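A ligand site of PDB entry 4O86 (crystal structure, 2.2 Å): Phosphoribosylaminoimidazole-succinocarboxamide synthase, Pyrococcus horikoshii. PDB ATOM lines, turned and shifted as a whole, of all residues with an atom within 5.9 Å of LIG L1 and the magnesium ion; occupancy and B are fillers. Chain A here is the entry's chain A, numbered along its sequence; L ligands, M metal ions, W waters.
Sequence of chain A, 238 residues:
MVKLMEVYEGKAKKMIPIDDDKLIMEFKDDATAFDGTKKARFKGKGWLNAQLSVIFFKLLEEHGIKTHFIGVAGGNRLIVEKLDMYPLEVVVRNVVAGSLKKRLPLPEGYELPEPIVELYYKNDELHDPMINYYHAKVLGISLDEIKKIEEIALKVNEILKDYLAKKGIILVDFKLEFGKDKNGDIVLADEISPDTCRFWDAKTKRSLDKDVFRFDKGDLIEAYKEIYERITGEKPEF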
ATOM      1  N   ALA A  12      19.127  -6.173   9.577  1.00  0.00           N
ATOM      2  CA  ALA A  12      17.838  -5.386   9.541  1.00  0.00           C
ATOM      3  C   ALA A  12      17.980  -3.951  10.093  1.00  0.00           C
ATOM      4  O   ALA A  12      17.041  -3.150  10.012  1.00  0.00           O
ATOM      5  CB  ALA A  12      16.740  -6.134  10.294  1.00  0.00           C
ATOM      6  N   LYS A  13      19.147  -3.651  10.667  1.00  0.00           N
ATOM      7  CA  LYS A  13      19.384  -2.355  11.303  1.00  0.00           C
ATOM      8  C   LYS A  13      20.806  -1.860  11.069  1.00  0.00           C
ATOM      9  O   LYS A  13      21.747  -2.657  11.014  1.00  0.00           O
ATOM     10  CB  LYS A  13      19.091  -2.411  12.818  1.00  0.00           C
ATOM     11  CG  LYS A  13      17.706  -2.901  13.207  1.00  0.00           C
ATOM     12  CD  LYS A  13      17.390  -2.669  14.682  1.00  0.00           C
ATOM     13  CE  LYS A  13      18.300  -3.403  15.648  1.00  0.00           C
ATOM     14  NZ  LYS A  13      18.496  -4.848  15.338  1.00  0.00           N
ATOM     15  N   LYS A  14      20.945  -0.541  10.926  1.00  0.00           N
ATOM     16  CA  LYS A  14      22.233   0.159  10.921  1.00  0.00           C
ATOM     17  C   LYS A  14      22.541   0.759  12.309  1.00  0.00           C
ATOM     18  O   LYS A  14      21.651   1.341  12.948  1.00  0.00           O
ATOM     19  CB  LYS A  14      22.247   1.260   9.858  1.00  0.00           C
ATOM     20  N   MET A  15      23.782   0.601  12.767  1.00  0.00           N
ATOM     21  CA  MET A  15      24.222   1.228  14.016  1.00  0.00           C
ATOM     22  C   MET A  15      25.299   2.250  13.674  1.00  0.00           C
ATOM     23  O   MET A  15      26.327   1.904  13.076  1.00  0.00           O
ATOM     24  CB  MET A  15      24.786   0.184  15.008  1.00  0.00           C
ATOM     25  CG  MET A  15      23.866  -0.990  15.337  1.00  0.00           C
ATOM     26  SD  MET A  15      22.292  -0.610  16.137  1.00  0.00           S
ATOM     27  CE  MET A  15      22.796  -0.001  17.747  1.00  0.00           C
ATOM     28  N   LEU A  23      24.621   5.862  20.372  1.00  0.00           N
ATOM     29  CA  LEU A  23      24.582   5.280  19.039  1.00  0.00           C
ATOM     30  C   LEU A  23      23.283   5.653  18.362  1.00  0.00           C
ATOM     31  O   LEU A  23      22.278   5.915  19.027  1.00  0.00           O
ATOM     32  CB  LEU A  23      24.644   3.751  19.145  1.00  0.00           C
ATOM     33  CG  LEU A  23      25.853   2.890  18.794  1.00  0.00           C
ATOM     34  CD1 LEU A  23      27.209   3.537  19.098  1.00  0.00           C
ATOM     35  CD2 LEU A  23      25.693   1.583  19.558  1.00  0.00           C
ATOM     36  N   MET A  25      20.447   3.971  16.197  1.00  0.00           N
ATOM     37  CA  MET A  25      19.917   2.683  15.747  1.00  0.00           C
ATOM     38  C   MET A  25      18.893   2.914  14.640  1.00  0.00           C
ATOM     39  O   MET A  25      17.774   3.387  14.898  1.00  0.00           O
ATOM     40  CB  MET A  25      19.314   1.891  16.923  1.00  0.00           C
ATOM     41  CG  MET A  25      18.715   0.544  16.530  1.00  0.00           C
ATOM     42  SD  MET A  25      18.436  -0.580  17.915  1.00  0.00           S
ATOM     43  CE  MET A  25      17.167   0.288  18.845  1.00  0.00           C
ATOM     44  N   HIS A  68      18.228   0.630  26.802  1.00  0.00           N
ATOM     45  CA  HIS A  68      19.166   1.547  26.152  1.00  0.00           C
ATOM     46  C   HIS A  68      18.480   2.705  25.467  1.00  0.00           C
ATOM     47  O   HIS A  68      19.158   3.576  24.917  1.00  0.00           O
ATOM     48  CB  HIS A  68      20.041   0.779  25.160  1.00  0.00           C
ATOM     49  CG  HIS A  68      19.285   0.259  23.933  1.00  0.00           C
ATOM     50  ND1 HIS A  68      19.922  -0.093  22.794  1.00  0.00           N
ATOM     51  CD2 HIS A  68      17.927   0.059  23.699  1.00  0.00           C
ATOM     52  CE1 HIS A  68      19.027  -0.510  21.877  1.00  0.00           C
ATOM     53  NE2 HIS A  68      17.801  -0.423  22.439  1.00  0.00           N
ATOM     54  N   VAL A  80      20.265   5.627  21.086  1.00  0.00           N
ATOM     55  CA  VAL A  80      20.415   4.636  22.144  1.00  0.00           C
ATOM     56  C   VAL A  80      21.771   4.718  22.839  1.00  0.00           C
ATOM     57  O   VAL A  80      22.754   5.113  22.215  1.00  0.00           O
ATOM     58  CB  VAL A  80      20.154   3.167  21.672  1.00  0.00           C
ATOM     59  CG1 VAL A  80      18.699   2.975  21.224  1.00  0.00           C
ATOM     60  CG2 VAL A  80      21.144   2.744  20.595  1.00  0.00           C
ATOM     61  N   GLU A  81      21.788   4.345  24.112  1.00  0.00           N
ATOM     62  CA  GLU A  81      23.001   4.247  24.894  1.00  0.00           C
ATOM     63  C   GLU A  81      23.867   3.109  24.352  1.00  0.00           C
ATOM     64  O   GLU A  81      23.383   2.004  24.132  1.00  0.00           O
ATOM     65  CB  GLU A  81      22.629   3.981  26.343  1.00  0.00           C
ATOM     66  CG  GLU A  81      23.807   3.925  27.311  1.00  0.00           C
ATOM     67  CD  GLU A  81      23.405   3.485  28.704  1.00  0.00           C
ATOM     68  OE1 GLU A  81      22.251   3.055  28.906  1.00  0.00           O
ATOM     69  OE2 GLU A  81      24.257   3.559  29.594  1.00  0.00           O
ATOM     70  N   LYS A  82      25.148   3.400  24.120  1.00  0.00           N
ATOM     71  CA  LYS A  82      26.115   2.370  23.758  1.00  0.00           C
ATOM     72  C   LYS A  82      26.388   1.482  24.977  1.00  0.00           C
ATOM     73  O   LYS A  82      26.576   1.974  26.081  1.00  0.00           O
ATOM     74  CB  LYS A  82      27.405   3.009  23.250  1.00  0.00           C
ATOM     75  CG  LYS A  82      28.384   2.039  22.590  1.00  0.00           C
ATOM     76  CD  LYS A  82      29.799   2.611  22.553  1.00  0.00           C
ATOM     77  CE  LYS A  82      30.705   1.774  21.676  1.00  0.00           C
ATOM     78  NZ  LYS A  82      32.152   1.961  22.000  1.00  0.00           N
ATOM     79  N   LEU A  83      26.385   0.170  24.759  1.00  0.00           N
ATOM     80  CA  LEU A  83      26.644  -0.784  25.820  1.00  0.00           C
ATOM     81  C   LEU A  83      27.729  -1.762  25.405  1.00  0.00           C
ATOM     82  O   LEU A  83      27.969  -1.954  24.229  1.00  0.00           O
ATOM     83  CB  LEU A  83      25.376  -1.588  26.115  1.00  0.00           C
ATOM     84  CG  LEU A  83      24.159  -0.813  26.606  1.00  0.00           C
ATOM     85  CD1 LEU A  83      22.901  -1.680  26.461  1.00  0.00           C
ATOM     86  CD2 LEU A  83      24.352  -0.332  28.035  1.00  0.00           C
ATOM     87  N   ASP A  84      28.392  -2.355  26.396  1.00  0.00           N
ATOM     88  CA  ASP A  84      29.213  -3.519  26.171  1.00  0.00           C
ATOM     89  C   ASP A  84      28.251  -4.706  26.064  1.00  0.00           C
ATOM     90  O   ASP A  84      27.705  -5.152  27.060  1.00  0.00           O
ATOM     91  CB  ASP A  84      30.183  -3.692  27.343  1.00  0.00           C
ATOM     92  CG  ASP A  84      31.124  -4.868  27.167  1.00  0.00           C
ATOM     93  OD1 ASP A  84      31.825  -5.192  28.144  1.00  0.00           O
ATOM     94  OD2 ASP A  84      31.171  -5.450  26.075  1.00  0.00           O
ATOM     95  N   MET A  85      28.025  -5.181  24.841  1.00  0.00           N
ATOM     96  CA  MET A  85      27.007  -6.203  24.592  1.00  0.00           C
ATOM     97  C   MET A  85      27.396  -7.593  25.095  1.00  0.00           C
ATOM     98  O   MET A  85      28.512  -8.025  24.909  1.00  0.00           O
ATOM     99  CB  MET A  85      26.634  -6.260  23.109  1.00  0.00           C
ATOM    100  CG  MET A  85      25.951  -5.001  22.593  1.00  0.00           C
ATOM    101  SD  MET A  85      24.321  -4.668  23.311  1.00  0.00           S
ATOM    102  CE  MET A  85      23.334  -5.934  22.498  1.00  0.00           C
ATOM    103  N   GLU A  89      21.423 -14.108  22.716  1.00  0.00           N
ATOM    104  CA  GLU A  89      20.044 -13.829  22.376  1.00  0.00           C
ATOM    105  C   GLU A  89      19.233 -14.602  23.394  1.00  0.00           C
ATOM    106  O   GLU A  89      19.429 -15.819  23.550  1.00  0.00           O
ATOM    107  CB  GLU A  89      19.748 -14.245  20.935  1.00  0.00           C
ATOM    108  CG  GLU A  89      20.564 -13.396  19.958  1.00  0.00           C
ATOM    109  CD  GLU A  89      20.124 -13.528  18.515  1.00  0.00           C
ATOM    110  OE1 GLU A  89      20.865 -13.020  17.633  1.00  0.00           O
ATOM    111  OE2 GLU A  89      19.067 -14.139  18.252  1.00  0.00           O
ATOM    112  N   LYS A 122      25.226 -15.765  20.466  1.00  0.00           N
ATOM    113  CA  LYS A 122      25.186 -14.924  19.267  1.00  0.00           C
ATOM    114  C   LYS A 122      26.525 -15.043  18.541  1.00  0.00           C
ATOM    115  O   LYS A 122      27.488 -14.375  18.910  1.00  0.00           O
ATOM    116  CB  LYS A 122      24.889 -13.487  19.638  1.00  0.00           C
ATOM    117  CG  LYS A 122      24.318 -12.660  18.510  1.00  0.00           C
ATOM    118  CD  LYS A 122      24.140 -11.203  18.931  1.00  0.00           C
ATOM    119  CE  LYS A 122      23.878 -10.337  17.707  1.00  0.00           C
ATOM    120  NZ  LYS A 122      22.692 -10.802  16.920  1.00  0.00           N
ATOM    121  N   ASP A 124      27.963 -16.021  14.484  1.00  0.00           N
ATOM    122  CA  ASP A 124      27.662 -16.353  13.082  1.00  0.00           C
ATOM    123  C   ASP A 124      28.352 -17.620  12.591  1.00  0.00           C
ATOM    124  O   ASP A 124      27.702 -18.460  11.979  1.00  0.00           O
ATOM    125  CB  ASP A 124      28.010 -15.170  12.182  1.00  0.00           C
ATOM    126  CG  ASP A 124      26.994 -14.061  12.281  1.00  0.00           C
ATOM    127  OD1 ASP A 124      25.789 -14.340  12.074  1.00  0.00           O
ATOM    128  OD2 ASP A 124      27.383 -12.907  12.577  1.00  0.00           O
ATOM    129  N   LYS A 175      12.561 -12.599  21.410  1.00  0.00           N
ATOM    130  CA  LYS A 175      13.997 -12.578  21.666  1.00  0.00           C
ATOM    131  C   LYS A 175      14.432 -11.204  22.213  1.00  0.00           C
ATOM    132  O   LYS A 175      14.040 -10.165  21.685  1.00  0.00           O
ATOM    133  CB  LYS A 175      14.766 -12.904  20.378  1.00  0.00           C
ATOM    134  CG  LYS A 175      16.289 -12.981  20.530  1.00  0.00           C
ATOM    135  CD  LYS A 175      16.990 -11.652  20.265  1.00  0.00           C
ATOM    136  CE  LYS A 175      16.904 -11.236  18.791  1.00  0.00           C
ATOM    137  NZ  LYS A 175      17.443  -9.861  18.529  1.00  0.00           N
ATOM    138  N   GLU A 177      18.030  -8.901  23.704  1.00  0.00           N
ATOM    139  CA  GLU A 177      19.475  -8.788  23.841  1.00  0.00           C
ATOM    140  C   GLU A 177      19.818  -7.779  24.947  1.00  0.00           C
ATOM    141  O   GLU A 177      19.018  -6.881  25.259  1.00  0.00           O
ATOM    142  CB  GLU A 177      20.098  -8.372  22.513  1.00  0.00           C
ATOM    143  CG  GLU A 177      19.977  -9.451  21.455  1.00  0.00           C
ATOM    144  CD  GLU A 177      20.662  -9.075  20.161  1.00  0.00           C
ATOM    145  OE1 GLU A 177      21.688  -8.374  20.232  1.00  0.00           O
ATOM    146  OE2 GLU A 177      20.179  -9.494  19.101  1.00  0.00           O
ATOM    147  N   ALA A 189      18.692  -4.162  25.491  1.00  0.00           N
ATOM    148  CA  ALA A 189      19.222  -3.527  24.285  1.00  0.00           C
ATOM    149  C   ALA A 189      18.471  -3.899  22.995  1.00  0.00           C
ATOM    150  O   ALA A 189      17.310  -4.325  23.029  1.00  0.00           O
ATOM    151  CB  ALA A 189      20.720  -3.810  24.162  1.00  0.00           C
ATOM    152  N   ASP A 190      19.142  -3.707  21.858  1.00  0.00           N
ATOM    153  CA  ASP A 190      18.600  -4.065  20.549  1.00  0.00           C
ATOM    154  C   ASP A 190      17.168  -3.552  20.307  1.00  0.00           C
ATOM    155  O   ASP A 190      16.876  -2.373  20.575  1.00  0.00           O
ATOM    156  CB  ASP A 190      18.708  -5.577  20.309  1.00  0.00           C
ATOM    157  CG  ASP A 190      18.701  -5.952  18.824  1.00  0.00           C
ATOM    158  OD1 ASP A 190      17.793  -6.709  18.429  1.00  0.00           O
ATOM    159  OD2 ASP A 190      19.592  -5.483  18.072  1.00  0.00           O
ATOM    160  N   GLU A 191      16.287  -4.427  19.822  1.00  0.00           N
ATOM    161  CA  GLU A 191      14.963  -4.020  19.374  1.00  0.00           C
ATOM    162  C   GLU A 191      13.894  -4.893  19.976  1.00  0.00           C
ATOM    163  O   GLU A 191      14.180  -6.008  20.439  1.00  0.00           O
ATOM    164  CB  GLU A 191      14.872  -4.082  17.828  1.00  0.00           C
ATOM    165  CG  GLU A 191      14.810  -5.493  17.241  1.00  0.00           C
ATOM    166  CD  GLU A 191      14.627  -5.539  15.730  1.00  0.00           C
ATOM    167  OE1 GLU A 191      13.547  -5.175  15.239  1.00  0.00           O
ATOM    168  OE2 GLU A 191      15.542  -5.977  15.009  1.00  0.00           O
HETATM  169  P1  LIG L   1      22.826  -8.348  13.808  1.00  0.00           P
HETATM  170  O1  LIG L   1      22.542  -8.806  12.401  1.00  0.00           O
HETATM  171  O2  LIG L   1      24.249  -8.538  14.270  1.00  0.00           O
HETATM  172  O3  LIG L   1      21.779  -8.788  14.828  1.00  0.00           O
HETATM  173  P2  LIG L   1      21.297  -5.930  13.830  1.00  0.00           P
HETATM  174  O4  LIG L   1      20.661  -5.764  12.472  1.00  0.00           O
HETATM  175  O5  LIG L   1      20.474  -6.496  14.955  1.00  0.00           O
HETATM  176  O6  LIG L   1      22.680  -6.743  13.688  1.00  0.00           O
HETATM  177  O7  LIG L   1      21.870  -4.496  14.311  1.00  0.00           O
HETATM  178  C1  LIG L   1      22.103  -4.204  15.692  1.00  0.00           C
HETATM  179  C2  LIG L   1      23.479  -4.662  16.208  1.00  0.00           C
HETATM  180  O8  LIG L   1      23.889  -3.803  17.286  1.00  0.00           O
HETATM  181  C3  LIG L   1      23.435  -6.044  16.841  1.00  0.00           C
HETATM  182  O9  LIG L   1      24.727  -6.638  16.718  1.00  0.00           O
HETATM  183  C4  LIG L   1      23.127  -5.773  18.305  1.00  0.00           C
HETATM  184  O10 LIG L   1      23.553  -6.818  19.168  1.00  0.00           O
HETATM  185  C5  LIG L   1      23.902  -4.493  18.545  1.00  0.00           C
HETATM  186  N1  LIG L   1      23.281  -3.603  19.562  1.00  0.00           N
HETATM  187  C6  LIG L   1      21.968  -3.464  19.846  1.00  0.00           C
HETATM  188  N2  LIG L   1      21.777  -2.548  20.817  1.00  0.00           N
HETATM  189  C7  LIG L   1      22.999  -2.053  21.160  1.00  0.00           C
HETATM  190  C8  LIG L   1      23.545  -1.056  22.119  1.00  0.00           C
HETATM  191  N3  LIG L   1      22.736  -0.344  22.942  1.00  0.00           N
HETATM  192  N4  LIG L   1      24.888  -0.881  22.163  1.00  0.00           N
HETATM  193  C9  LIG L   1      25.735  -1.553  21.361  1.00  0.00           C
HETATM  194  N5  LIG L   1      25.313  -2.461  20.474  1.00  0.00           N
HETATM  195  C10 LIG L   1      23.988  -2.758  20.331  1.00  0.00           C
HETATM  196  P1  LG2 L   2      19.025 -11.396  15.229  1.00  0.00           P
HETATM  197  O1  LG2 L   2      19.539 -12.797  15.458  1.00  0.00           O
HETATM  198  O2  LG2 L   2      17.526 -11.318  15.400  1.00  0.00           O
HETATM  199  O3  LG2 L   2      19.654 -10.466  16.231  1.00  0.00           O
HETATM  200  O4  LG2 L   2      19.399 -10.985  13.812  1.00  0.00           O
HETATM  201 MG    MG M   1      19.795  -8.490  15.223  1.00  0.00          MG
HETATM  202  O   HOH W   1      20.720  -7.905  16.936  1.00  0.00           O
HETATM  203  O   HOH W   2      17.168  -8.252  15.980  1.00  0.00           O
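The magnesium ion is bound by water W1 (2.0 Å), O3 of LIG L1 (2.0 Å), O5 of LIG L1 (2.1 Å) and O3 of LG2 L2 (2.2 Å). The magnesium ion has four donor atoms within binding distance. Slightly farther from the magnesium ion lies water W2 (2.7 Å).
The side-chain amino group (NZ) of Lys 13 is in salt-bridge range of the side-chain carboxylate (OD2) of Asp 190, 3.0 Å away. The side-chain amino group (NZ) of Lys 13 lies within salt-bridge range of the side-chain carboxylate (OE2) of Glu 191 (3.2 Å). The side-chain amino group (NZ) of Lys 175 is in salt-bridge range of the side-chain carboxylate (OE2) of Glu 177, 2.8 Å away. The backbone NH (N) of Glu 81 sits at hydrogen-bond distance from the backbone carbonyl oxygen (O) of His 68. A ring nitrogen (NE2) of His 68 sits at hydrogen-bond distance from the backbone carbonyl oxygen (O) of Asp 190, at 2.9 Å. The side-chain amino group of Lys 122 is in salt-bridge range of the side-chain carboxylate of Glu 89 (3.0 Å). The side-chain carboxylate (OD1) of Asp 190 lies within salt-bridge range of the side-chain amino group (NZ) of Lys 175, at 3.2 Å. O of Val 80 lies within hydrogen-bond range of N of Leu 23 (2.7 Å).
An oxygen (O8) of LIG L1 sits close to the side-chain sulfur (SD) of Met 15 (3.8 Å). The side-chain sulfur (SD) of Met 85 sits close to a nitrogen (N5) of LIG L1. CD2 of Leu 23 touches C9 of LIG L1, at 3.6 Å. CA of Lys 82 touches N4 of LIG L1, at 3.8 Å. Ala 189 touches LIG L1 (CB to N2, 3.7 Å). Of the 21 residues printed, 13 come within 4 Å of LIG L1.
Lys 13 touches the magnesium ion.
Water W1 bridges OE2 of Glu 177 (2.7 Å) and OD2 of Asp 190 (2.9 Å). Water W2 lies within hydrogen-bond range of the side-chain carboxylate (OE2) of Glu 191, the side-chain carboxylate (OD1) of Asp 190 and the side-chain amino group (NZ) of Lys 175.
The backbone NH of Lys 13 is in hydrogen-bond range of an oxygen (O4) of LIG L1 (3.2 Å). The side-chain amino group of Lys 13 is in salt-bridge range of an oxygen (O4) of LIG L1 (3.7 Å). The side-chain carboxylate (OE1) of Glu 177 sits at hydrogen-bond distance from an oxygen (O10) of LIG L1 (2.7 Å). The backbone carbonyl oxygen (O) of Glu 81 sits at hydrogen-bond distance from a nitrogen (N3) of LIG L1, 2.7 Å away. N3 of LIG L1 is in hydrogen-bond range of ND1 of His 68. NZ of Lys 122 lies within salt-bridge range of O2 of LIG L1 (3.8 Å). A nitrogen (N2) of LIG L1 is in hydrogen-bond range of the backbone NH (N) of Asp 190 (3.1 Å). The backbone NH (N) of Leu 83 is in hydrogen-bond range of a nitrogen (N4) of LIG L1 (3.2 Å). The backbone NH of Ala 12 is in hydrogen-bond range of an oxygen (O4) of LIG L1, 3.3 Å away.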
